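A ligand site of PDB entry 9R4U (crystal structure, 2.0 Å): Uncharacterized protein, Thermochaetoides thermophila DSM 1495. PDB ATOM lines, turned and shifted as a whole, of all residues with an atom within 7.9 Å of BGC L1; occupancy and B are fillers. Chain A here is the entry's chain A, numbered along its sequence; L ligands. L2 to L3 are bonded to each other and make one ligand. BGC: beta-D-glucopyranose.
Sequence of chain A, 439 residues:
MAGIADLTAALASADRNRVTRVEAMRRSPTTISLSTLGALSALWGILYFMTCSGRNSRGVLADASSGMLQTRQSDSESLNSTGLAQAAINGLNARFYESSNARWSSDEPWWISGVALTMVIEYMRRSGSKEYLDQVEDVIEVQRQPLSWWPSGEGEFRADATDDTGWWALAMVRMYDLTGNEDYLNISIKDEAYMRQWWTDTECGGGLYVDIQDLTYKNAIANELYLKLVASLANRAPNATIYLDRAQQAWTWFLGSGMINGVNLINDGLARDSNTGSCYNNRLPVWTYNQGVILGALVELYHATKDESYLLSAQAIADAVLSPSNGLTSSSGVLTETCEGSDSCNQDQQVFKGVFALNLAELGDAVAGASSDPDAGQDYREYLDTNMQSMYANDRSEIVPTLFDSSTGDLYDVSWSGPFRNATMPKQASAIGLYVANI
The guanidinium group (NH2) of Arg 103 sits at hydrogen-bond distance from the backbone carbonyl oxygen (O) of Glu 108 (3.1 Å).
The indole nitrogen (NE1) of Trp 110 sits at hydrogen-bond distance from the side-chain amide oxygen (OE1) of Gln 143 (3.0 Å).
Residues that only touch BGC L1: Arg 103, Glu 108, Pro 109 and Trp 149.
Hydrophobic or aromatic side chains that line BGC L1: Trp 110 and Trp 149.
The side-chain carboxylate of Asp 160 lies within hydrogen-bond range of an oxygen (O6) of BGC L1 (3.1 Å).
The side-chain carboxylate of Asp 164 is in hydrogen-bond range of an oxygen (O1) of BGC L2 (2.6 Å).
O2 of BGC L2 sits at hydrogen-bond distance from N of Asp 164, 3.5 Å away.
N of Trp 110 is in hydrogen-bond range of O1 of BGC L1.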
ATOM      1  N   ARG A 103      17.978  -2.450 -25.564  1.00  0.00           N
ATOM      2  CA  ARG A 103      19.261  -3.143 -25.515  1.00  0.00           C
ATOM      3  C   ARG A 103      19.606  -3.542 -26.939  1.00  0.00           C
ATOM      4  O   ARG A 103      18.714  -3.592 -27.799  1.00  0.00           O
ATOM      5  CB  ARG A 103      19.151  -4.364 -24.598  1.00  0.00           C
ATOM      6  CG  ARG A 103      20.244  -5.304 -24.647  1.00  0.00           C
ATOM      7  CD  ARG A 103      19.976  -6.473 -23.778  1.00  0.00           C
ATOM      8  NE  ARG A 103      21.123  -7.351 -23.858  1.00  0.00           N
ATOM      9  CZ  ARG A 103      21.405  -8.290 -22.964  1.00  0.00           C
ATOM     10  NH1 ARG A 103      20.582  -8.560 -21.956  1.00  0.00           N
ATOM     11  NH2 ARG A 103      22.521  -8.991 -23.115  1.00  0.00           N
ATOM     12  N   SER A 105      21.030  -6.718 -29.154  1.00  0.00           N
ATOM     13  CA  SER A 105      21.290  -8.152 -29.142  1.00  0.00           C
ATOM     14  C   SER A 105      21.272  -8.801 -27.766  1.00  0.00           C
ATOM     15  O   SER A 105      22.352  -8.994 -27.174  1.00  0.00           O
ATOM     16  CB  SER A 105      22.674  -8.427 -29.753  1.00  0.00           C
ATOM     17  OG  SER A 105      22.731  -8.036 -31.113  1.00  0.00           O
ATOM     18  N   SER A 106      20.095  -9.153 -27.240  1.00  0.00           N
ATOM     19  CA  SER A 106      20.074  -9.948 -26.014  1.00  0.00           C
ATOM     20  C   SER A 106      20.763 -11.312 -26.162  1.00  0.00           C
ATOM     21  O   SER A 106      20.998 -11.981 -25.153  1.00  0.00           O
ATOM     22  CB  SER A 106      18.629 -10.141 -25.485  1.00  0.00           C
ATOM     23  OG  SER A 106      17.802  -8.993 -25.670  1.00  0.00           O
ATOM     24  N   ASP A 107      21.120 -11.720 -27.385  1.00  0.00           N
ATOM     25  CA  ASP A 107      21.840 -12.984 -27.584  1.00  0.00           C
ATOM     26  C   ASP A 107      23.352 -12.798 -27.583  1.00  0.00           C
ATOM     27  O   ASP A 107      24.103 -13.731 -27.917  1.00  0.00           O
ATOM     28  CB  ASP A 107      21.326 -13.652 -28.888  1.00  0.00           C
ATOM     29  CG  ASP A 107      21.589 -12.840 -30.152  1.00  0.00           C
ATOM     30  OD1 ASP A 107      21.727 -13.465 -31.196  1.00  0.00           O
ATOM     31  OD2 ASP A 107      21.852 -11.622 -30.097  1.00  0.00           O
ATOM     32  N   GLU A 108      23.828 -11.648 -27.125  1.00  0.00           N
ATOM     33  CA  GLU A 108      25.225 -11.234 -27.122  1.00  0.00           C
ATOM     34  C   GLU A 108      25.469 -10.728 -25.711  1.00  0.00           C
ATOM     35  O   GLU A 108      24.530 -10.258 -25.052  1.00  0.00           O
ATOM     36  CB  GLU A 108      25.376 -10.115 -28.159  1.00  0.00           C
ATOM     37  CG  GLU A 108      25.514 -10.587 -29.585  1.00  0.00           C
ATOM     38  CD  GLU A 108      26.749 -11.519 -29.945  1.00  0.00           C
ATOM     39  OE1 GLU A 108      27.209 -12.452 -29.231  1.00  0.00           O
ATOM     40  OE2 GLU A 108      27.021 -11.452 -31.155  1.00  0.00           O
ATOM     41  N   PRO A 109      26.693 -10.820 -25.207  1.00  0.00           N
ATOM     42  CA  PRO A 109      26.912 -10.449 -23.792  1.00  0.00           C
ATOM     43  C   PRO A 109      26.445  -9.033 -23.475  1.00  0.00           C
ATOM     44  O   PRO A 109      26.640  -8.083 -24.264  1.00  0.00           O
ATOM     45  CB  PRO A 109      28.423 -10.569 -23.601  1.00  0.00           C
ATOM     46  CG  PRO A 109      28.857 -11.619 -24.698  1.00  0.00           C
ATOM     47  CD  PRO A 109      27.898 -11.340 -25.866  1.00  0.00           C
ATOM     48  N   TRP A 110      25.848  -8.909 -22.291  1.00  0.00           N
ATOM     49  CA  TRP A 110      25.332  -7.622 -21.783  1.00  0.00           C
ATOM     50  C   TRP A 110      26.415  -6.553 -21.713  1.00  0.00           C
ATOM     51  O   TRP A 110      26.157  -5.406 -22.096  1.00  0.00           O
ATOM     52  CB  TRP A 110      24.731  -7.868 -20.404  1.00  0.00           C
ATOM     53  CG  TRP A 110      24.104  -6.656 -19.669  1.00  0.00           C
ATOM     54  CD1 TRP A 110      22.910  -6.057 -19.966  1.00  0.00           C
ATOM     55  CD2 TRP A 110      24.658  -5.934 -18.547  1.00  0.00           C
ATOM     56  NE1 TRP A 110      22.686  -5.017 -19.096  1.00  0.00           N
ATOM     57  CE2 TRP A 110      23.716  -4.929 -18.197  1.00  0.00           C
ATOM     58  CE3 TRP A 110      25.830  -6.045 -17.800  1.00  0.00           C
ATOM     59  CZ2 TRP A 110      23.927  -4.029 -17.146  1.00  0.00           C
ATOM     60  CZ3 TRP A 110      26.055  -5.150 -16.739  1.00  0.00           C
ATOM     61  CH2 TRP A 110      25.058  -4.166 -16.392  1.00  0.00           C
ATOM     62  N   TRP A 111      27.649  -6.905 -21.305  1.00  0.00           N
ATOM     63  CA  TRP A 111      28.653  -5.853 -21.209  1.00  0.00           C
ATOM     64  C   TRP A 111      28.911  -5.193 -22.566  1.00  0.00           C
ATOM     65  O   TRP A 111      29.301  -4.001 -22.615  1.00  0.00           O
ATOM     66  CB  TRP A 111      29.943  -6.402 -20.622  1.00  0.00           C
ATOM     67  CG  TRP A 111      30.738  -7.331 -21.576  1.00  0.00           C
ATOM     68  CD1 TRP A 111      30.532  -8.651 -21.774  1.00  0.00           C
ATOM     69  CD2 TRP A 111      31.869  -6.967 -22.349  1.00  0.00           C
ATOM     70  NE1 TRP A 111      31.492  -9.168 -22.674  1.00  0.00           N
ATOM     71  CE2 TRP A 111      32.349  -8.142 -23.010  1.00  0.00           C
ATOM     72  CE3 TRP A 111      32.562  -5.737 -22.532  1.00  0.00           C
ATOM     73  CZ2 TRP A 111      33.453  -8.127 -23.881  1.00  0.00           C
ATOM     74  CZ3 TRP A 111      33.695  -5.732 -23.385  1.00  0.00           C
ATOM     75  CH2 TRP A 111      34.132  -6.916 -24.040  1.00  0.00           C
ATOM     76  N   ILE A 112      28.602  -5.902 -23.656  1.00  0.00           N
ATOM     77  CA  ILE A 112      28.876  -5.310 -24.962  1.00  0.00           C
ATOM     78  C   ILE A 112      27.766  -4.335 -25.352  1.00  0.00           C
ATOM     79  O   ILE A 112      28.039  -3.349 -26.055  1.00  0.00           O
ATOM     80  CB  ILE A 112      29.204  -6.378 -26.036  1.00  0.00           C
ATOM     81  CG1 ILE A 112      30.451  -7.181 -25.636  1.00  0.00           C
ATOM     82  CG2 ILE A 112      29.415  -5.803 -27.476  1.00  0.00           C
ATOM     83  CD1 ILE A 112      30.555  -8.610 -26.388  1.00  0.00           C
ATOM     84  N   SER A 113      26.565  -4.475 -24.799  1.00  0.00           N
ATOM     85  CA  SER A 113      25.600  -3.353 -24.905  1.00  0.00           C
ATOM     86  C   SER A 113      26.152  -2.109 -24.236  1.00  0.00           C
ATOM     87  O   SER A 113      25.965  -0.992 -24.725  1.00  0.00           O
ATOM     88  CB  SER A 113      24.253  -3.759 -24.305  1.00  0.00           C
ATOM     89  OG  SER A 113      23.457  -4.353 -25.324  1.00  0.00           O
ATOM     90  N   GLN A 143      18.353  -0.552 -18.580  1.00  0.00           N
ATOM     91  CA  GLN A 143      19.494  -1.380 -18.174  1.00  0.00           C
ATOM     92  C   GLN A 143      19.998  -1.018 -16.778  1.00  0.00           C
ATOM     93  O   GLN A 143      20.723  -1.811 -16.175  1.00  0.00           O
ATOM     94  CB  GLN A 143      20.610  -1.204 -19.225  1.00  0.00           C
ATOM     95  CG  GLN A 143      20.273  -1.809 -20.607  1.00  0.00           C
ATOM     96  CD  GLN A 143      19.501  -3.127 -20.571  1.00  0.00           C
ATOM     97  OE1 GLN A 143      19.944  -4.084 -19.886  1.00  0.00           O
ATOM     98  NE2 GLN A 143      18.461  -3.227 -21.368  1.00  0.00           N
ATOM     99  N   LEU A 147      19.378  -6.253 -12.086  1.00  0.00           N
ATOM    100  CA  LEU A 147      19.544  -7.275 -13.102  1.00  0.00           C
ATOM    101  C   LEU A 147      18.896  -8.586 -12.684  1.00  0.00           C
ATOM    102  O   LEU A 147      19.084  -9.066 -11.557  1.00  0.00           O
ATOM    103  CB  LEU A 147      21.051  -7.510 -13.381  1.00  0.00           C
ATOM    104  CG  LEU A 147      21.752  -6.206 -13.730  1.00  0.00           C
ATOM    105  CD1 LEU A 147      23.278  -6.401 -13.726  1.00  0.00           C
ATOM    106  CD2 LEU A 147      21.295  -5.678 -15.080  1.00  0.00           C
ATOM    107  N   SER A 148      18.139  -9.183 -13.620  1.00  0.00           N
ATOM    108  CA  SER A 148      17.478 -10.438 -13.310  1.00  0.00           C
ATOM    109  C   SER A 148      18.476 -11.525 -12.913  1.00  0.00           C
ATOM    110  O   SER A 148      18.125 -12.394 -12.103  1.00  0.00           O
ATOM    111  CB  SER A 148      16.616 -10.876 -14.501  1.00  0.00           C
ATOM    112  OG  SER A 148      17.430 -11.175 -15.638  1.00  0.00           O
ATOM    113  N   TRP A 149      19.726 -11.491 -13.429  1.00  0.00           N
ATOM    114  CA  TRP A 149      20.711 -12.498 -13.037  1.00  0.00           C
ATOM    115  C   TRP A 149      21.575 -12.066 -11.862  1.00  0.00           C
ATOM    116  O   TRP A 149      22.407 -12.858 -11.417  1.00  0.00           O
ATOM    117  CB  TRP A 149      21.624 -12.871 -14.214  1.00  0.00           C
ATOM    118  CG  TRP A 149      22.446 -11.728 -14.737  1.00  0.00           C
ATOM    119  CD1 TRP A 149      23.742 -11.422 -14.407  1.00  0.00           C
ATOM    120  CD2 TRP A 149      22.043 -10.741 -15.706  1.00  0.00           C
ATOM    121  NE1 TRP A 149      24.153 -10.287 -15.093  1.00  0.00           N
ATOM    122  CE2 TRP A 149      23.138  -9.864 -15.904  1.00  0.00           C
ATOM    123  CE3 TRP A 149      20.852 -10.504 -16.402  1.00  0.00           C
ATOM    124  CZ2 TRP A 149      23.079  -8.800 -16.759  1.00  0.00           C
ATOM    125  CZ3 TRP A 149      20.802  -9.462 -17.260  1.00  0.00           C
ATOM    126  CH2 TRP A 149      21.897  -8.603 -17.433  1.00  0.00           C
ATOM    127  N   TRP A 150      21.433 -10.850 -11.345  1.00  0.00           N
ATOM    128  CA  TRP A 150      22.190 -10.425 -10.162  1.00  0.00           C
ATOM    129  C   TRP A 150      21.389  -9.376  -9.393  1.00  0.00           C
ATOM    130  O   TRP A 150      21.802  -8.216  -9.270  1.00  0.00           O
ATOM    131  CB  TRP A 150      23.553  -9.878 -10.554  1.00  0.00           C
ATOM    132  CG  TRP A 150      24.463  -9.783  -9.371  1.00  0.00           C
ATOM    133  CD1 TRP A 150      24.979  -8.664  -8.813  1.00  0.00           C
ATOM    134  CD2 TRP A 150      24.924 -10.889  -8.570  1.00  0.00           C
ATOM    135  NE1 TRP A 150      25.761  -8.997  -7.719  1.00  0.00           N
ATOM    136  CE2 TRP A 150      25.731 -10.357  -7.545  1.00  0.00           C
ATOM    137  CE3 TRP A 150      24.744 -12.269  -8.628  1.00  0.00           C
ATOM    138  CZ2 TRP A 150      26.370 -11.153  -6.603  1.00  0.00           C
ATOM    139  CZ3 TRP A 150      25.368 -13.077  -7.670  1.00  0.00           C
ATOM    140  CH2 TRP A 150      26.168 -12.518  -6.674  1.00  0.00           C
ATOM    141  N   ALA A 159      26.778  -5.544 -11.156  1.00  0.00           N
ATOM    142  CA  ALA A 159      26.490  -6.844 -11.768  1.00  0.00           C
ATOM    143  C   ALA A 159      27.255  -7.963 -11.050  1.00  0.00           C
ATOM    144  O   ALA A 159      27.872  -7.758 -10.008  1.00  0.00           O
ATOM    145  CB  ALA A 159      26.798  -6.784 -13.274  1.00  0.00           C
ATOM    146  N   ASP A 160      27.229  -9.180 -11.617  1.00  0.00           N
ATOM    147  CA  ASP A 160      27.916 -10.270 -10.940  1.00  0.00           C
ATOM    148  C   ASP A 160      29.402 -10.345 -11.327  1.00  0.00           C
ATOM    149  O   ASP A 160      30.047 -11.331 -10.992  1.00  0.00           O
ATOM    150  CB  ASP A 160      27.300 -11.644 -11.260  1.00  0.00           C
ATOM    151  CG  ASP A 160      27.274 -11.955 -12.768  1.00  0.00           C
ATOM    152  OD1 ASP A 160      27.781 -11.173 -13.590  1.00  0.00           O
ATOM    153  OD2 ASP A 160      26.774 -13.031 -13.137  1.00  0.00           O
ATOM    154  N   ALA A 161      29.933  -9.370 -12.075  1.00  0.00           N
ATOM    155  CA  ALA A 161      31.361  -9.314 -12.334  1.00  0.00           C
ATOM    156  C   ALA A 161      31.798  -7.869 -12.244  1.00  0.00           C
ATOM    157  O   ALA A 161      31.049  -6.978 -12.657  1.00  0.00           O
ATOM    158  CB  ALA A 161      31.707  -9.939 -13.732  1.00  0.00           C
ATOM    159  N   ASP A 164      32.076  -6.285 -15.930  1.00  0.00           N
ATOM    160  CA  ASP A 164      30.754  -5.906 -16.478  1.00  0.00           C
ATOM    161  C   ASP A 164      30.294  -4.545 -15.907  1.00  0.00           C
ATOM    162  O   ASP A 164      29.844  -3.646 -16.632  1.00  0.00           O
ATOM    163  CB  ASP A 164      29.686  -6.959 -16.135  1.00  0.00           C
ATOM    164  CG  ASP A 164      29.859  -8.227 -16.920  1.00  0.00           C
ATOM    165  OD1 ASP A 164      31.020  -8.516 -17.297  1.00  0.00           O
ATOM    166  OD2 ASP A 164      28.908  -8.981 -17.113  1.00  0.00           O
ATOM    167  N   GLN A 213      31.313 -13.851  -7.292  1.00  0.00           N
ATOM    168  CA  GLN A 213      30.911 -15.043  -6.560  1.00  0.00           C
ATOM    169  C   GLN A 213      32.094 -15.932  -6.196  1.00  0.00           C
ATOM    170  O   GLN A 213      31.964 -16.772  -5.294  1.00  0.00           O
ATOM    171  CB  GLN A 213      29.933 -15.851  -7.436  1.00  0.00           C
ATOM    172  CG  GLN A 213      28.744 -15.010  -7.906  1.00  0.00           C
ATOM    173  CD  GLN A 213      27.619 -15.827  -8.532  1.00  0.00           C
ATOM    174  OE1 GLN A 213      26.856 -16.519  -7.829  1.00  0.00           O
ATOM    175  NE2 GLN A 213      27.506 -15.749  -9.854  1.00  0.00           N
HETATM  176  C2  BGC L   1      23.306 -12.187 -19.908  1.00  0.00           C
HETATM  177  C3  BGC L   1      22.988 -12.794 -18.539  1.00  0.00           C
HETATM  178  C4  BGC L   1      24.221 -13.451 -17.941  1.00  0.00           C
HETATM  179  C5  BGC L   1      25.379 -12.446 -17.866  1.00  0.00           C
HETATM  180  C6  BGC L   1      26.679 -13.006 -17.323  1.00  0.00           C
HETATM  181  C1  BGC L   1      24.583 -11.324 -19.873  1.00  0.00           C
HETATM  182  O1  BGC L   1      25.018 -11.090 -21.173  1.00  0.00           O
HETATM  183  O2  BGC L   1      22.185 -11.416 -20.355  1.00  0.00           O
HETATM  184  O3  BGC L   1      21.942 -13.751 -18.665  1.00  0.00           O
HETATM  185  O4  BGC L   1      23.911 -14.012 -16.673  1.00  0.00           O
HETATM  186  O5  BGC L   1      25.678 -11.991 -19.195  1.00  0.00           O
HETATM  187  O6  BGC L   1      26.462 -13.799 -16.156  1.00  0.00           O
HETATM  188  C2  BGC L   2      33.787  -8.686 -19.276  1.00  0.00           C
HETATM  189  C3  BGC L   2      34.704  -8.422 -20.460  1.00  0.00           C
HETATM  190  C4  BGC L   2      35.576  -9.652 -20.771  1.00  0.00           C
HETATM  191  C5  BGC L   2      34.754 -10.912 -20.951  1.00  0.00           C
HETATM  192  C6  BGC L   2      35.607 -12.160 -21.164  1.00  0.00           C
HETATM  193  C1  BGC L   2      33.010  -9.967 -19.605  1.00  0.00           C
HETATM  194  O1  BGC L   2      32.150 -10.380 -18.658  1.00  0.00           O
HETATM  195  O2  BGC L   2      32.946  -7.535 -19.033  1.00  0.00           O
HETATM  196  O3  BGC L   2      35.548  -7.293 -20.238  1.00  0.00           O
HETATM  197  O4  BGC L   2      36.204  -9.473 -22.026  1.00  0.00           O
HETATM  198  O5  BGC L   2      33.996 -11.113 -19.772  1.00  0.00           O
HETATM  199  O6  BGC L   2      36.082 -12.804 -19.994  1.00  0.00           O
HETATM  200  C2  BGC L   3      38.501 -12.939 -19.170  1.00  0.00           C
HETATM  201  C3  BGC L   3      39.445 -11.784 -19.455  1.00  0.00           C
HETATM  202  C4  BGC L   3      39.965 -11.928 -20.909  1.00  0.00           C
HETATM  203  C5  BGC L   3      38.904 -12.379 -21.950  1.00  0.00           C
HETATM  204  C6  BGC L   3      39.470 -12.963 -23.248  1.00  0.00           C
HETATM  205  C1  BGC L   3      37.482 -12.571 -20.239  1.00  0.00           C
HETATM  206  O2  BGC L   3      37.979 -13.046 -17.854  1.00  0.00           O
HETATM  207  O3  BGC L   3      40.458 -11.603 -18.479  1.00  0.00           O
HETATM  208  O4  BGC L   3      40.583 -10.735 -21.409  1.00  0.00           O
HETATM  209  O5  BGC L   3      37.999 -13.360 -21.399  1.00  0.00           O
HETATM  210  O6  BGC L   3      38.412 -13.014 -24.205  1.00  0.00           O
